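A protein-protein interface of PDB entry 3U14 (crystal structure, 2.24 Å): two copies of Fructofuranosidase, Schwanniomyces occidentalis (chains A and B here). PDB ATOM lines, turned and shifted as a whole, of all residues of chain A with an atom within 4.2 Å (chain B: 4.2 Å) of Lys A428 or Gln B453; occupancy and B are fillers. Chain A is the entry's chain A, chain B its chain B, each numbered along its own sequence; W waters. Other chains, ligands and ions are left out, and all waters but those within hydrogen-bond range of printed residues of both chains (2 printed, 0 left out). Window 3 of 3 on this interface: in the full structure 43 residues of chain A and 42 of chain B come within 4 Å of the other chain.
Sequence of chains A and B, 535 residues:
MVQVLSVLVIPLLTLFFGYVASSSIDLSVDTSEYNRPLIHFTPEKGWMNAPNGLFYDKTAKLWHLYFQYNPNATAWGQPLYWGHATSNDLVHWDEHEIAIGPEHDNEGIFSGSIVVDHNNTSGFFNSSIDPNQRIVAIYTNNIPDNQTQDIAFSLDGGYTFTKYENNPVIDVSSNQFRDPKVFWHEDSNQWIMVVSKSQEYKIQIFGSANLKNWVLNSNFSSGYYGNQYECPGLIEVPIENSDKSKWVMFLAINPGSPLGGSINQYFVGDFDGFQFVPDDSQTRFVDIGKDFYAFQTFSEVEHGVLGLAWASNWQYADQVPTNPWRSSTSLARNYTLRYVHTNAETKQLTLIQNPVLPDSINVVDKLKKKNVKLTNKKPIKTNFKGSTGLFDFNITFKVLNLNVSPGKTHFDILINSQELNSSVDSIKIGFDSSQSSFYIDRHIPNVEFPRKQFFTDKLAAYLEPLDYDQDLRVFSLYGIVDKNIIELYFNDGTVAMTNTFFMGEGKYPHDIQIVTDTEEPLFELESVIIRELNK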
ATOM      1  N   ASP A 412     -22.489  23.179  25.123  1.00  0.00           N
ATOM      2  CA  ASP A 412     -21.151  22.741  24.741  1.00  0.00           C
ATOM      3  C   ASP A 412     -20.366  22.067  25.862  1.00  0.00           C
ATOM      4  O   ASP A 412     -20.368  22.542  26.997  1.00  0.00           O
ATOM      5  CB  ASP A 412     -20.372  23.932  24.195  1.00  0.00           C
ATOM      6  CG  ASP A 412     -21.042  24.544  22.981  1.00  0.00           C
ATOM      7  OD1 ASP A 412     -21.939  25.369  23.173  1.00  0.00           O
ATOM      8  OD2 ASP A 412     -20.696  24.193  21.837  1.00  0.00           O
ATOM      9  N   ILE A 413     -19.709  20.960  25.524  1.00  0.00           N
ATOM     10  CA  ILE A 413     -18.779  20.257  26.404  1.00  0.00           C
ATOM     11  C   ILE A 413     -17.366  20.706  26.044  1.00  0.00           C
ATOM     12  O   ILE A 413     -16.945  20.613  24.886  1.00  0.00           O
ATOM     13  CB  ILE A 413     -18.923  18.707  26.266  1.00  0.00           C
ATOM     14  CG1 ILE A 413     -20.383  18.276  26.489  1.00  0.00           C
ATOM     15  CG2 ILE A 413     -17.992  17.971  27.228  1.00  0.00           C
ATOM     16  CD1 ILE A 413     -20.749  16.960  25.862  1.00  0.00           C
ATOM     17  N   LEU A 414     -16.650  21.241  27.030  1.00  0.00           N
ATOM     18  CA  LEU A 414     -15.304  21.732  26.805  1.00  0.00           C
ATOM     19  C   LEU A 414     -14.274  20.837  27.465  1.00  0.00           C
ATOM     20  O   LEU A 414     -14.402  20.476  28.643  1.00  0.00           O
ATOM     21  CB  LEU A 414     -15.155  23.161  27.316  1.00  0.00           C
ATOM     22  CG  LEU A 414     -16.144  24.201  26.791  1.00  0.00           C
ATOM     23  CD1 LEU A 414     -15.865  25.503  27.505  1.00  0.00           C
ATOM     24  CD2 LEU A 414     -16.020  24.382  25.289  1.00  0.00           C
ATOM     25  N   ILE A 427     -10.808  21.554  23.153  1.00  0.00           N
ATOM     26  CA  ILE A 427     -11.658  21.109  22.074  1.00  0.00           C
ATOM     27  C   ILE A 427     -13.088  21.141  22.592  1.00  0.00           C
ATOM     28  O   ILE A 427     -13.314  21.071  23.797  1.00  0.00           O
ATOM     29  CB  ILE A 427     -11.250  19.701  21.549  1.00  0.00           C
ATOM     30  CG1 ILE A 427     -11.360  18.652  22.653  1.00  0.00           C
ATOM     31  CG2 ILE A 427      -9.831  19.730  20.986  1.00  0.00           C
ATOM     32  CD1 ILE A 427     -11.161  17.238  22.159  1.00  0.00           C
ATOM     33  N   LYS A 428     -14.045  21.231  21.679  1.00  0.00           N
ATOM     34  CA  LYS A 428     -15.438  21.506  22.011  1.00  0.00           C
ATOM     35  C   LYS A 428     -16.332  20.418  21.404  1.00  0.00           C
ATOM     36  O   LYS A 428     -16.131  20.025  20.254  1.00  0.00           O
ATOM     37  CB  LYS A 428     -15.769  22.891  21.444  1.00  0.00           C
ATOM     38  CG  LYS A 428     -17.129  23.493  21.771  1.00  0.00           C
ATOM     39  CD  LYS A 428     -17.094  25.046  21.560  1.00  0.00           C
ATOM     40  CE  LYS A 428     -17.502  25.508  20.151  1.00  0.00           C
ATOM     41  NZ  LYS A 428     -18.958  25.910  20.099  1.00  0.00           N
ATOM     42  N   ILE A 429     -17.291  19.913  22.178  1.00  0.00           N
ATOM     43  CA  ILE A 429     -18.304  18.989  21.667  1.00  0.00           C
ATOM     44  C   ILE A 429     -19.658  19.546  22.085  1.00  0.00           C
ATOM     45  O   ILE A 429     -19.919  19.729  23.285  1.00  0.00           O
ATOM     46  CB  ILE A 429     -18.187  17.543  22.260  1.00  0.00           C
ATOM     47  CG1 ILE A 429     -16.816  16.918  21.988  1.00  0.00           C
ATOM     48  CG2 ILE A 429     -19.303  16.635  21.746  1.00  0.00           C
ATOM     49  CD1 ILE A 429     -15.805  17.231  23.077  1.00  0.00           C
ATOM     50  N   ASP A 432     -26.758  21.410  18.926  1.00  0.00           N
ATOM     51  CA  ASP A 432     -27.607  22.558  18.633  1.00  0.00           C
ATOM     52  C   ASP A 432     -29.018  22.023  18.416  1.00  0.00           C
ATOM     53  O   ASP A 432     -29.222  21.088  17.631  1.00  0.00           O
ATOM     54  CB  ASP A 432     -27.081  23.353  17.434  1.00  0.00           C
ATOM     55  CG  ASP A 432     -27.853  24.659  17.191  1.00  0.00           C
ATOM     56  OD1 ASP A 432     -29.090  24.597  16.983  1.00  0.00           O
ATOM     57  OD2 ASP A 432     -27.232  25.745  17.195  1.00  0.00           O
ATOM     58  N   TYR A 439     -21.957  18.290  17.250  1.00  0.00           N
ATOM     59  CA  TYR A 439     -20.786  18.742  16.516  1.00  0.00           C
ATOM     60  C   TYR A 439     -19.551  18.654  17.392  1.00  0.00           C
ATOM     61  O   TYR A 439     -19.655  18.584  18.617  1.00  0.00           O
ATOM     62  CB  TYR A 439     -20.968  20.180  16.039  1.00  0.00           C
ATOM     63  CG  TYR A 439     -21.388  21.142  17.142  1.00  0.00           C
ATOM     64  CD1 TYR A 439     -20.440  21.754  17.953  1.00  0.00           C
ATOM     65  CD2 TYR A 439     -22.735  21.450  17.352  1.00  0.00           C
ATOM     66  CE1 TYR A 439     -20.810  22.636  18.953  1.00  0.00           C
ATOM     67  CE2 TYR A 439     -23.130  22.328  18.354  1.00  0.00           C
ATOM     68  CZ  TYR A 439     -22.160  22.914  19.156  1.00  0.00           C
ATOM     69  OH  TYR A 439     -22.511  23.802  20.141  1.00  0.00           O
ATOM     70  N   ILE A 440     -18.393  18.648  16.745  1.00  0.00           N
ATOM     71  CA  ILE A 440     -17.109  18.796  17.402  1.00  0.00           C
ATOM     72  C   ILE A 440     -16.370  19.951  16.728  1.00  0.00           C
ATOM     73  O   ILE A 440     -16.564  20.250  15.537  1.00  0.00           O
ATOM     74  CB  ILE A 440     -16.231  17.498  17.312  1.00  0.00           C
ATOM     75  CG1 ILE A 440     -14.984  17.617  18.214  1.00  0.00           C
ATOM     76  CG2 ILE A 440     -15.812  17.195  15.835  1.00  0.00           C
ATOM     77  CD1 ILE A 440     -14.318  16.316  18.532  1.00  0.00           C
ATOM     78  N   ASP A 441     -15.525  20.606  17.504  1.00  0.00           N
ATOM     79  CA  ASP A 441     -14.578  21.539  16.968  1.00  0.00           C
ATOM     80  C   ASP A 441     -13.248  21.191  17.619  1.00  0.00           C
ATOM     81  O   ASP A 441     -13.087  21.349  18.825  1.00  0.00           O
ATOM     82  CB  ASP A 441     -15.004  22.981  17.283  1.00  0.00           C
ATOM     83  CG  ASP A 441     -14.101  24.004  16.645  1.00  0.00           C
ATOM     84  OD1 ASP A 441     -13.117  23.613  15.966  1.00  0.00           O
ATOM     85  OD2 ASP A 441     -14.377  25.210  16.810  1.00  0.00           O
ATOM     86  N   LYS A 458     -14.087  21.160  12.098  1.00  0.00           N
ATOM     87  CA  LYS A 458     -15.515  21.185  12.423  1.00  0.00           C
ATOM     88  C   LYS A 458     -16.277  20.067  11.724  1.00  0.00           C
ATOM     89  O   LYS A 458     -16.373  20.053  10.485  1.00  0.00           O
ATOM     90  CB  LYS A 458     -16.113  22.545  12.043  1.00  0.00           C
ATOM     91  CG  LYS A 458     -15.637  23.702  12.914  1.00  0.00           C
ATOM     92  CD  LYS A 458     -16.272  25.030  12.494  1.00  0.00           C
ATOM     93  CE  LYS A 458     -15.857  26.161  13.421  1.00  0.00           C
ATOM     94  NZ  LYS A 458     -16.560  27.457  13.077  1.00  0.00           N
ATOM     95  N   ARG B 451     -24.885  29.569  14.629  1.00  0.00           N
ATOM     96  CA  ARG B 451     -24.759  28.259  13.993  1.00  0.00           C
ATOM     97  C   ARG B 451     -23.533  28.113  13.113  1.00  0.00           C
ATOM     98  O   ARG B 451     -23.496  27.256  12.228  1.00  0.00           O
ATOM     99  CB  ARG B 451     -26.029  27.883  13.239  1.00  0.00           C
ATOM    100  CG  ARG B 451     -27.260  28.087  14.076  1.00  0.00           C
ATOM    101  CD  ARG B 451     -28.279  27.047  13.807  1.00  0.00           C
ATOM    102  NE  ARG B 451     -29.557  27.636  13.414  1.00  0.00           N
ATOM    103  CZ  ARG B 451     -30.257  28.514  14.133  1.00  0.00           C
ATOM    104  NH1 ARG B 451     -29.826  28.938  15.311  1.00  0.00           N
ATOM    105  NH2 ARG B 451     -31.403  28.965  13.655  1.00  0.00           N
ATOM    106  N   LYS B 452     -22.521  28.931  13.380  1.00  0.00           N
ATOM    107  CA  LYS B 452     -21.230  28.779  12.727  1.00  0.00           C
ATOM    108  C   LYS B 452     -20.460  27.484  13.111  1.00  0.00           C
ATOM    109  O   LYS B 452     -19.439  27.188  12.493  1.00  0.00           O
ATOM    110  CB  LYS B 452     -20.356  30.046  12.896  1.00  0.00           C
ATOM    111  CG  LYS B 452     -19.265  30.154  11.827  1.00  0.00           C
ATOM    112  CD  LYS B 452     -18.509  31.480  11.742  1.00  0.00           C
ATOM    113  CE  LYS B 452     -17.317  31.294  10.776  1.00  0.00           C
ATOM    114  NZ  LYS B 452     -16.396  32.456  10.616  1.00  0.00           N
ATOM    115  N   GLN B 453     -20.941  26.725  14.101  1.00  0.00           N
ATOM    116  CA  GLN B 453     -20.353  25.409  14.437  1.00  0.00           C
ATOM    117  C   GLN B 453     -20.445  24.471  13.240  1.00  0.00           C
ATOM    118  O   GLN B 453     -19.687  23.516  13.141  1.00  0.00           O
ATOM    119  CB  GLN B 453     -21.059  24.709  15.606  1.00  0.00           C
ATOM    120  CG  GLN B 453     -21.134  25.488  16.908  1.00  0.00           C
ATOM    121  CD  GLN B 453     -22.246  26.531  16.909  1.00  0.00           C
ATOM    122  OE1 GLN B 453     -23.267  26.386  16.231  1.00  0.00           O
ATOM    123  NE2 GLN B 453     -22.045  27.598  17.680  1.00  0.00           N
ATOM    124  N   PHE B 454     -21.377  24.769  12.343  1.00  0.00           N
ATOM    125  CA  PHE B 454     -21.662  23.913  11.205  1.00  0.00           C
ATOM    126  C   PHE B 454     -21.053  24.467   9.909  1.00  0.00           C
ATOM    127  O   PHE B 454     -21.118  23.820   8.869  1.00  0.00           O
ATOM    128  CB  PHE B 454     -23.176  23.737  11.063  1.00  0.00           C
ATOM    129  CG  PHE B 454     -23.858  23.228  12.318  1.00  0.00           C
ATOM    130  CD1 PHE B 454     -24.647  24.083  13.091  1.00  0.00           C
ATOM    131  CD2 PHE B 454     -23.719  21.904  12.713  1.00  0.00           C
ATOM    132  CE1 PHE B 454     -25.270  23.627  14.258  1.00  0.00           C
ATOM    133  CE2 PHE B 454     -24.341  21.417  13.869  1.00  0.00           C
ATOM    134  CZ  PHE B 454     -25.123  22.275  14.652  1.00  0.00           C
ATOM    135  N   PHE B 455     -20.468  25.665   9.992  1.00  0.00           N
ATOM    136  CA  PHE B 455     -19.854  26.341   8.856  1.00  0.00           C
ATOM    137  C   PHE B 455     -18.430  25.791   8.668  1.00  0.00           C
ATOM    138  O   PHE B 455     -17.456  26.416   9.088  1.00  0.00           O
ATOM    139  CB  PHE B 455     -19.851  27.860   9.109  1.00  0.00           C
ATOM    140  CG  PHE B 455     -19.650  28.708   7.879  1.00  0.00           C
ATOM    141  CD1 PHE B 455     -20.726  29.028   7.049  1.00  0.00           C
ATOM    142  CD2 PHE B 455     -18.411  29.260   7.589  1.00  0.00           C
ATOM    143  CE1 PHE B 455     -20.561  29.837   5.921  1.00  0.00           C
ATOM    144  CE2 PHE B 455     -18.235  30.066   6.466  1.00  0.00           C
ATOM    145  CZ  PHE B 455     -19.326  30.351   5.628  1.00  0.00           C
HETATM  146  O   HOH W   1     -19.569  21.139  11.253  1.00  0.00           O
HETATM  147  O   HOH W   2     -17.945  22.700  15.288  1.00  0.00           O
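No position is printed for both chains.
Of the 8 pairs that touch across the chains among the printed residues, none has its exchanged pair printed and touching as well.
The side-chain amino group (NZ) of Lys A458 sits at hydrogen-bond distance from the backbone carbonyl oxygen (O) of Lys B452, 2.9 Å away.
Of the printed residues of chain B, Tyr A439 touches Gln B453 (3.5 Å) and Phe B454 (3.7 Å).
Of the printed residues of chain A, Lys B452 touches Lys A458 (2.9 Å).
Of the printed residues of chain A, Phe B454 touches Asp A432 (3.6 Å) and Tyr A439 (3.7 Å).
Asp A412 touches none of the printed residues of chain B.
The nearest printed residue of chain B that does not touch Lys A428 is Lys B452 (7.3 Å).
Among the printed residues, pairs that only touch across the chains: Lys A428 with Gln B453, Asp A432 with Arg B451, Asp A432 with Phe B454, Tyr A439 with Gln B453, Tyr A439 with Phe B454, Lys A458 with Gln B453 and Lys A458 with Phe B455.
The side-chain carboxylate of Asp A412 lies within salt-bridge range of the side-chain amino group of Lys A428.
The side-chain hydroxyl (OH) of Tyr A439 sits at hydrogen-bond distance from the side-chain carboxylate (OD2) of Asp A412 (2.5 Å).
The backbone NH of Asp A441 lies within hydrogen-bond range of the backbone carbonyl oxygen of Lys A428, 2.9 Å away.
Water W2 lies within hydrogen-bond range of the backbone carbonyl oxygen of Ile A440 (2.8 Å) and the backbone carbonyl oxygen of Gln B453 (2.9 Å).
Water W1 bridges the backbone carbonyl oxygen (O) of Gln B453 (3.0 Å) and the backbone carbonyl oxygen (O) of Lys A458 (3.5 Å).
Of the 5 printed residues of chain B, 5 touch a printed residue of chain A.
Printed residues of chain B that touch a printed residue of chain A: Arg B451, Lys B452, Gln B453, Phe B454 and Phe B455.
Printed residues of chain A that touch a printed residue of chain B: Lys A428, Asp A432, Tyr A439 and Lys A458.
Among the printed residues, no Asp or Glu carboxylate lies within 4 Å of a Lys or Arg side-chain nitrogen of the other chain.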
